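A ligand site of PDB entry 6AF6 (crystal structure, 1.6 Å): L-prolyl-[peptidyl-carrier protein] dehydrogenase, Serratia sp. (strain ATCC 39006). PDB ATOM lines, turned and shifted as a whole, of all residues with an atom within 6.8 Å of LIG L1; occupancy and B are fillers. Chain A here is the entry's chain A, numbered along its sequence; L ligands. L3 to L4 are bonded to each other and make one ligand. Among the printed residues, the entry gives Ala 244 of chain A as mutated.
An oxygen (O9) of LG2 L2 is in hydrogen-bond range of an oxygen (O1) of LIG L1.
An oxygen (O11) of LG2 L2 is in hydrogen-bond range of a nitrogen (N1) of LG3 L3, 2.9 Å away.
The side-chain sulfur of Met 241 sits close to an oxygen (O2) of LIG L1, 3.6 Å away.
Residues that only touch LIG L1: Phe 364 and Ala 91.
Hydrophobic or aromatic side chains that line LIG L1: Ala 91, Met 241 and Phe 364.
Within 4 Å of LIG L1: Ala 91, Asn 125, Met 241, Phe 364 and Ser 365.
An oxygen (O1) of LIG L1 is in hydrogen-bond range of the backbone NH (N) of Ser 365 (2.9 Å).
N1 of LIG L1 lies within hydrogen-bond range of OD1 of Asn 125, 3.5 Å away.
A nitrogen (N7) of LG2 L2 sits at hydrogen-bond distance from the backbone carbonyl oxygen (O) of Asn 125 (2.9 Å).
N7 of LG2 L2 sits at hydrogen-bond distance from OD1 of Asn 125, 3.3 Å away.
N of Thr 128 is in hydrogen-bond range of O7 of LG2 L2 (2.8 Å).
OG1 of Thr 128 sits at hydrogen-bond distance from N6 of LG2 L2 (2.9 Å).
An oxygen (O8) of LG2 L2 lies within hydrogen-bond range of the backbone NH (N) of Thr 160, at 3.0 Å.
N8 of LG2 L2 is in hydrogen-bond range of OG1 of Thr 160.
N of Ala 127 lies within hydrogen-bond range of O7 of LG2 L2.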
ATOM      1  N   PHE A  87       3.020  21.619  24.356  1.00  0.00           N
ATOM      2  CA  PHE A  87       3.050  20.734  23.202  1.00  0.00           C
ATOM      3  C   PHE A  87       2.536  21.455  21.956  1.00  0.00           C
ATOM      4  O   PHE A  87       3.095  21.320  20.879  1.00  0.00           O
ATOM      5  CB  PHE A  87       2.231  19.434  23.497  1.00  0.00           C
ATOM      6  CG  PHE A  87       2.249  18.441  22.351  1.00  0.00           C
ATOM      7  CD1 PHE A  87       3.315  17.613  22.210  1.00  0.00           C
ATOM      8  CD2 PHE A  87       1.213  18.400  21.449  1.00  0.00           C
ATOM      9  CE1 PHE A  87       3.321  16.699  21.074  1.00  0.00           C
ATOM     10  CE2 PHE A  87       1.225  17.477  20.396  1.00  0.00           C
ATOM     11  CZ  PHE A  87       2.305  16.696  20.224  1.00  0.00           C
ATOM     12  N   CYS A  90       5.275  23.753  20.670  1.00  0.00           N
ATOM     13  CA  CYS A  90       6.396  23.056  20.051  1.00  0.00           C
ATOM     14  C   CYS A  90       5.985  22.395  18.750  1.00  0.00           C
ATOM     15  O   CYS A  90       6.811  22.265  17.828  1.00  0.00           O
ATOM     16  CB  CYS A  90       6.975  22.058  21.065  1.00  0.00           C
ATOM     17  SG  CYS A  90       7.743  22.910  22.502  1.00  0.00           S
ATOM     18  N   ALA A  91       4.721  21.966  18.613  1.00  0.00           N
ATOM     19  CA  ALA A  91       4.263  21.419  17.342  1.00  0.00           C
ATOM     20  C   ALA A  91       4.279  22.503  16.272  1.00  0.00           C
ATOM     21  O   ALA A  91       4.751  22.297  15.156  1.00  0.00           O
ATOM     22  CB  ALA A  91       2.866  20.831  17.483  1.00  0.00           C
ATOM     23  N   HIS A  92       3.804  23.689  16.614  1.00  0.00           N
ATOM     24  CA  HIS A  92       3.852  24.809  15.678  1.00  0.00           C
ATOM     25  C   HIS A  92       5.281  25.127  15.277  1.00  0.00           C
ATOM     26  O   HIS A  92       5.578  25.289  14.088  1.00  0.00           O
ATOM     27  CB  HIS A  92       3.160  25.984  16.388  1.00  0.00           C
ATOM     28  CG  HIS A  92       3.413  27.329  15.786  1.00  0.00           C
ATOM     29  ND1 HIS A  92       2.538  27.897  14.870  1.00  0.00           N
ATOM     30  CD2 HIS A  92       4.401  28.236  15.989  1.00  0.00           C
ATOM     31  CE1 HIS A  92       2.978  29.105  14.540  1.00  0.00           C
ATOM     32  NE2 HIS A  92       4.068  29.368  15.247  1.00  0.00           N
ATOM     33  N   CYS A  94       8.070  23.066  15.487  1.00  0.00           N
ATOM     34  CA  CYS A  94       8.906  22.062  14.823  1.00  0.00           C
ATOM     35  C   CYS A  94       8.325  21.586  13.527  1.00  0.00           C
ATOM     36  O   CYS A  94       9.058  21.223  12.593  1.00  0.00           O
ATOM     37  CB  CYS A  94       9.132  20.847  15.766  1.00  0.00           C
ATOM     38  SG  CYS A  94      10.015  21.292  17.240  1.00  0.00           S
ATOM     39  N   ALA A  95       7.011  21.502  13.425  1.00  0.00           N
ATOM     40  CA  ALA A  95       6.418  20.918  12.239  1.00  0.00           C
ATOM     41  C   ALA A  95       5.949  21.984  11.271  1.00  0.00           C
ATOM     42  O   ALA A  95       5.507  21.624  10.152  1.00  0.00           O
ATOM     43  CB  ALA A  95       5.253  20.013  12.622  1.00  0.00           C
ATOM     44  N   ASN A 125       0.277  21.198  11.207  1.00  0.00           N
ATOM     45  CA  ASN A 125       0.917  20.369  10.184  1.00  0.00           C
ATOM     46  C   ASN A 125       0.014  19.175   9.922  1.00  0.00           C
ATOM     47  O   ASN A 125      -0.441  18.519  10.863  1.00  0.00           O
ATOM     48  CB  ASN A 125       2.313  19.956  10.678  1.00  0.00           C
ATOM     49  CG  ASN A 125       2.694  18.534  10.305  1.00  0.00           C
ATOM     50  OD1 ASN A 125       2.505  17.590  11.060  1.00  0.00           O
ATOM     51  ND2 ASN A 125       3.273  18.394   9.174  1.00  0.00           N
ATOM     52  N   ALA A 127      -0.264  15.759   7.978  1.00  0.00           N
ATOM     53  CA  ALA A 127       0.314  14.684   7.187  1.00  0.00           C
ATOM     54  C   ALA A 127      -0.475  13.389   7.344  1.00  0.00           C
ATOM     55  O   ALA A 127      -0.843  12.745   6.340  1.00  0.00           O
ATOM     56  CB  ALA A 127       1.783  14.468   7.599  1.00  0.00           C
ATOM     57  N   THR A 128      -0.736  12.990   8.606  1.00  0.00           N
ATOM     58  CA  THR A 128      -1.426  11.735   8.875  1.00  0.00           C
ATOM     59  C   THR A 128      -2.797  11.651   8.251  1.00  0.00           C
ATOM     60  O   THR A 128      -3.591  12.602   8.264  1.00  0.00           O
ATOM     61  CB  THR A 128      -1.513  11.556  10.406  1.00  0.00           C
ATOM     62  OG1 THR A 128      -0.186  11.591  10.861  1.00  0.00           O
ATOM     63  CG2 THR A 128      -2.205  10.220  10.761  1.00  0.00           C
ATOM     64  N   PHE A 158      -5.909  13.640  13.214  1.00  0.00           N
ATOM     65  CA  PHE A 158      -5.005  13.771  14.386  1.00  0.00           C
ATOM     66  C   PHE A 158      -4.174  15.053  14.307  1.00  0.00           C
ATOM     67  O   PHE A 158      -2.994  15.098  14.689  1.00  0.00           O
ATOM     68  CB  PHE A 158      -4.046  12.549  14.525  1.00  0.00           C
ATOM     69  CG  PHE A 158      -4.746  11.237  14.651  1.00  0.00           C
ATOM     70  CD1 PHE A 158      -6.036  11.098  15.158  1.00  0.00           C
ATOM     71  CD2 PHE A 158      -4.070  10.086  14.226  1.00  0.00           C
ATOM     72  CE1 PHE A 158      -6.621   9.828  15.303  1.00  0.00           C
ATOM     73  CE2 PHE A 158      -4.710   8.814  14.389  1.00  0.00           C
ATOM     74  CZ  PHE A 158      -5.915   8.714  14.908  1.00  0.00           C
ATOM     75  N   THR A 160      -2.807  18.309  15.349  1.00  0.00           N
ATOM     76  CA  THR A 160      -2.575  19.226  16.493  1.00  0.00           C
ATOM     77  C   THR A 160      -2.762  20.669  16.019  1.00  0.00           C
ATOM     78  O   THR A 160      -2.255  21.047  14.951  1.00  0.00           O
ATOM     79  CB  THR A 160      -1.175  18.974  17.002  1.00  0.00           C
ATOM     80  OG1 THR A 160      -1.181  17.627  17.528  1.00  0.00           O
ATOM     81  CG2 THR A 160      -0.855  19.964  18.152  1.00  0.00           C
ATOM     82  N   PHE A 237       8.993  16.588   5.150  1.00  0.00           N
ATOM     83  CA  PHE A 237       8.315  15.991   6.306  1.00  0.00           C
ATOM     84  C   PHE A 237       9.338  15.289   7.183  1.00  0.00           C
ATOM     85  O   PHE A 237       9.310  15.399   8.436  1.00  0.00           O
ATOM     86  CB  PHE A 237       7.253  14.999   5.851  1.00  0.00           C
ATOM     87  CG  PHE A 237       6.514  14.330   6.997  1.00  0.00           C
ATOM     88  CD1 PHE A 237       5.580  15.061   7.728  1.00  0.00           C
ATOM     89  CD2 PHE A 237       6.790  13.024   7.366  1.00  0.00           C
ATOM     90  CE1 PHE A 237       4.911  14.491   8.818  1.00  0.00           C
ATOM     91  CE2 PHE A 237       6.109  12.439   8.460  1.00  0.00           C
ATOM     92  CZ  PHE A 237       5.167  13.178   9.149  1.00  0.00           C
ATOM     93  N   MET A 241      10.273  16.021  11.107  1.00  0.00           N
ATOM     94  CA  MET A 241      10.111  15.058  12.219  1.00  0.00           C
ATOM     95  C   MET A 241      11.387  14.890  12.998  1.00  0.00           C
ATOM     96  O   MET A 241      11.320  14.551  14.193  1.00  0.00           O
ATOM     97  CB  MET A 241       9.610  13.677  11.726  1.00  0.00           C
ATOM     98  CG  MET A 241       8.134  13.699  11.263  1.00  0.00           C
ATOM     99  SD  MET A 241       6.899  14.349  12.487  1.00  0.00           S
ATOM    100  CE  MET A 241       6.507  16.046  11.920  1.00  0.00           C
ATOM    101  N   ALA A 244      11.001  17.699  15.465  1.00  0.00           N
ATOM    102  CA  ALA A 244       9.952  17.284  16.389  1.00  0.00           C
ATOM    103  C   ALA A 244      10.435  16.204  17.348  1.00  0.00           C
ATOM    104  O   ALA A 244      10.190  16.290  18.574  1.00  0.00           O
ATOM    105  CB  ALA A 244       8.721  16.839  15.607  1.00  0.00           C
ATOM    106  N   LEU A 248      11.390  18.722  20.339  1.00  0.00           N
ATOM    107  CA  LEU A 248      10.133  18.683  21.070  1.00  0.00           C
ATOM    108  C   LEU A 248      10.202  17.699  22.235  1.00  0.00           C
ATOM    109  O   LEU A 248       9.698  17.991  23.321  1.00  0.00           O
ATOM    110  CB  LEU A 248       8.984  18.352  20.126  1.00  0.00           C
ATOM    111  CG  LEU A 248       7.573  18.520  20.653  1.00  0.00           C
ATOM    112  CD1 LEU A 248       6.658  18.764  19.455  1.00  0.00           C
ATOM    113  CD2 LEU A 248       7.090  17.257  21.385  1.00  0.00           C
ATOM    114  N   ILE A 363       3.889   7.881  20.729  1.00  0.00           N
ATOM    115  CA  ILE A 363       3.123   7.758  19.475  1.00  0.00           C
ATOM    116  C   ILE A 363       3.451   8.885  18.499  1.00  0.00           C
ATOM    117  O   ILE A 363       3.682   8.658  17.297  1.00  0.00           O
ATOM    118  CB  ILE A 363       1.628   7.736  19.777  1.00  0.00           C
ATOM    119  CG1 ILE A 363       1.272   6.591  20.750  1.00  0.00           C
ATOM    120  CG2 ILE A 363       0.771   7.615  18.495  1.00  0.00           C
ATOM    121  CD1 ILE A 363      -0.105   6.752  21.354  1.00  0.00           C
ATOM    122  N   PHE A 364       3.501  10.135  18.983  1.00  0.00           N
ATOM    123  CA  PHE A 364       3.582  11.110  17.911  1.00  0.00           C
ATOM    124  C   PHE A 364       5.035  11.256  17.392  1.00  0.00           C
ATOM    125  O   PHE A 364       6.031  10.742  17.946  1.00  0.00           O
ATOM    126  CB  PHE A 364       2.961  12.449  18.310  1.00  0.00           C
ATOM    127  CG  PHE A 364       3.378  12.931  19.659  1.00  0.00           C
ATOM    128  CD1 PHE A 364       4.692  13.216  19.913  1.00  0.00           C
ATOM    129  CD2 PHE A 364       2.462  13.092  20.659  1.00  0.00           C
ATOM    130  CE1 PHE A 364       5.098  13.640  21.160  1.00  0.00           C
ATOM    131  CE2 PHE A 364       2.835  13.523  21.930  1.00  0.00           C
ATOM    132  CZ  PHE A 364       4.156  13.816  22.182  1.00  0.00           C
ATOM    133  N   SER A 365       5.090  11.844  16.190  1.00  0.00           N
ATOM    134  CA  SER A 365       6.295  11.931  15.376  1.00  0.00           C
ATOM    135  C   SER A 365       6.868  10.565  15.019  1.00  0.00           C
ATOM    136  O   SER A 365       8.056  10.473  14.674  1.00  0.00           O
ATOM    137  CB  SER A 365       7.354  12.809  15.992  1.00  0.00           C
ATOM    138  OG  SER A 365       7.970  12.196  17.116  1.00  0.00           O
ATOM    139  N   GLY A 366       6.038   9.534  15.089  1.00  0.00           N
ATOM    140  CA  GLY A 366       6.463   8.195  14.717  1.00  0.00           C
ATOM    141  C   GLY A 366       6.441   7.351  15.964  1.00  0.00           C
ATOM    142  O   GLY A 366       7.037   7.738  16.976  1.00  0.00           O
HETATM  143  N1  LIG L   1       3.287  16.719  14.355  1.00  0.00           N
HETATM  144  C1  LIG L   1       3.965  15.457  14.661  1.00  0.00           C
HETATM  145  C2  LIG L   1       3.423  14.200  13.951  1.00  0.00           C
HETATM  146  O1  LIG L   1       3.136  13.156  14.530  1.00  0.00           O
HETATM  147  C3  LIG L   1       3.825  15.385  16.173  1.00  0.00           C
HETATM  148  C4  LIG L   1       4.132  16.864  16.575  1.00  0.00           C
HETATM  149  C5  LIG L   1       3.452  17.681  15.460  1.00  0.00           C
HETATM  150  O2  LIG L   1       3.324  14.202  12.718  1.00  0.00           O
HETATM  151  P1  LG2 L   2      -0.540   2.988  13.317  1.00  0.00           P
HETATM  152  O1  LG2 L   2      -1.805   2.389  12.992  1.00  0.00           O
HETATM  153  O2  LG2 L   2       0.397   3.270  12.296  1.00  0.00           O
HETATM  154  O3  LG2 L   2       0.222   2.035  14.381  1.00  0.00           O
HETATM  155  C1  LG2 L   2      -0.529   1.075  15.154  1.00  0.00           C
HETATM  156  C2  LG2 L   2       0.489   0.136  15.833  1.00  0.00           C
HETATM  157  O4  LG2 L   2       1.170  -0.599  14.791  1.00  0.00           O
HETATM  158  C3  LG2 L   2       1.599   0.856  16.610  1.00  0.00           C
HETATM  159  O5  LG2 L   2       2.025   0.017  17.692  1.00  0.00           O
HETATM  160  C4  LG2 L   2       2.713   0.930  15.566  1.00  0.00           C
HETATM  161  O6  LG2 L   2       3.997   1.020  16.140  1.00  0.00           O
HETATM  162  C5  LG2 L   2       2.549  -0.454  14.925  1.00  0.00           C
HETATM  163  N1  LG2 L   2       3.186  -0.570  13.619  1.00  0.00           N
HETATM  164  C6  LG2 L   2       2.818   0.059  12.438  1.00  0.00           C
HETATM  165  N2  LG2 L   2       3.642  -0.196  11.445  1.00  0.00           N
HETATM  166  C7  LG2 L   2       4.640  -0.973  12.020  1.00  0.00           C
HETATM  167  C8  LG2 L   2       5.831  -1.541  11.504  1.00  0.00           C
HETATM  168  N3  LG2 L   2       6.219  -1.410  10.235  1.00  0.00           N
HETATM  169  N4  LG2 L   2       6.603  -2.278  12.359  1.00  0.00           N
HETATM  170  C9  LG2 L   2       6.187  -2.425  13.624  1.00  0.00           C
HETATM  171  N5  LG2 L   2       5.086  -1.953  14.214  1.00  0.00           N
HETATM  172  C10 LG2 L   2       4.356  -1.228  13.345  1.00  0.00           C
HETATM  173  N6  LG2 L   2      -0.122  13.759  12.753  1.00  0.00           N
HETATM  174  C11 LG2 L   2      -0.035  14.848  11.918  1.00  0.00           C
HETATM  175  O7  LG2 L   2       0.008  14.755  10.680  1.00  0.00           O
HETATM  176  N7  LG2 L   2      -0.042  16.092  12.451  1.00  0.00           N
HETATM  177  C12 LG2 L   2      -0.092  16.376  13.834  1.00  0.00           C
HETATM  178  O8  LG2 L   2      -0.139  17.543  14.252  1.00  0.00           O
HETATM  179  C13 LG2 L   2      -0.141  15.210  14.695  1.00  0.00           C
HETATM  180  N8  LG2 L   2      -0.175  15.405  15.998  1.00  0.00           N
HETATM  181  C14 LG2 L   2      -0.344  14.314  16.813  1.00  0.00           C
HETATM  182  C15 LG2 L   2      -0.397  14.518  18.188  1.00  0.00           C
HETATM  183  C16 LG2 L   2      -0.530  13.436  19.049  1.00  0.00           C
HETATM  184  C17 LG2 L   2      -0.599  13.698  20.539  1.00  0.00           C
HETATM  185  C18 LG2 L   2      -0.530  12.138  18.545  1.00  0.00           C
HETATM  186  C19 LG2 L   2      -0.687  10.935  19.479  1.00  0.00           C
HETATM  187  C20 LG2 L   2      -0.491  11.933  17.172  1.00  0.00           C
HETATM  188  C21 LG2 L   2      -0.328  13.003  16.310  1.00  0.00           C
HETATM  189  N9  LG2 L   2      -0.224  12.828  14.903  1.00  0.00           N
HETATM  190  C22 LG2 L   2      -0.190  13.932  14.063  1.00  0.00           C
HETATM  191  C23 LG2 L   2      -0.382  11.467  14.319  1.00  0.00           C
HETATM  192  C24 LG2 L   2       0.823  10.536  14.521  1.00  0.00           C
HETATM  193  O9  LG2 L   2       1.824  10.940  13.605  1.00  0.00           O
HETATM  194  C25 LG2 L   2       0.370   9.086  14.267  1.00  0.00           C
HETATM  195  O10 LG2 L   2      -0.523   8.792  15.335  1.00  0.00           O
HETATM  196  C26 LG2 L   2       1.542   8.117  14.276  1.00  0.00           C
HETATM  197  O11 LG2 L   2       2.396   8.350  13.162  1.00  0.00           O
HETATM  198  C27 LG2 L   2       1.097   6.673  14.367  1.00  0.00           C
HETATM  199  O12 LG2 L   2       0.083   6.395  13.346  1.00  0.00           O
HETATM  200  P2  LG2 L   2      -1.246   5.761  13.679  1.00  0.00           P
HETATM  201  O13 LG2 L   2      -1.895   6.456  14.866  1.00  0.00           O
HETATM  202  O14 LG2 L   2      -2.002   5.620  12.437  1.00  0.00           O
HETATM  203  O15 LG2 L   2      -0.785   4.270  14.234  1.00  0.00           O
HETATM  204  N1  LG3 L   3       3.659   9.280  10.667  1.00  0.00           N
HETATM  205  C1  LG3 L   3       5.027   9.755  10.609  1.00  0.00           C
HETATM  206  C2  LG3 L   3       6.144   8.706  10.698  1.00  0.00           C
HETATM  207  O1  LG3 L   3       5.911   7.484  10.634  1.00  0.00           O
HETATM  208  C3  LG3 L   3       5.057  10.774  11.754  1.00  0.00           C
HETATM  209  C4  LG3 L   3       3.699  11.461  11.549  1.00  0.00           C
HETATM  210  C5  LG3 L   3       2.737  10.418  10.874  1.00  0.00           C
HETATM  211  N1  LG4 L   4       7.377   9.207  10.757  1.00  0.00           N
HETATM  212  C1  LG4 L   4       8.547   8.441  10.377  1.00  0.00           C
HETATM  213  C2  LG4 L   4       9.576   9.419   9.797  1.00  0.00           C
HETATM  214  O1  LG4 L   4      10.259  10.129  10.542  1.00  0.00           O
HETATM  215  O2  LG4 L   4       9.735   9.556   8.579  1.00  0.00           O
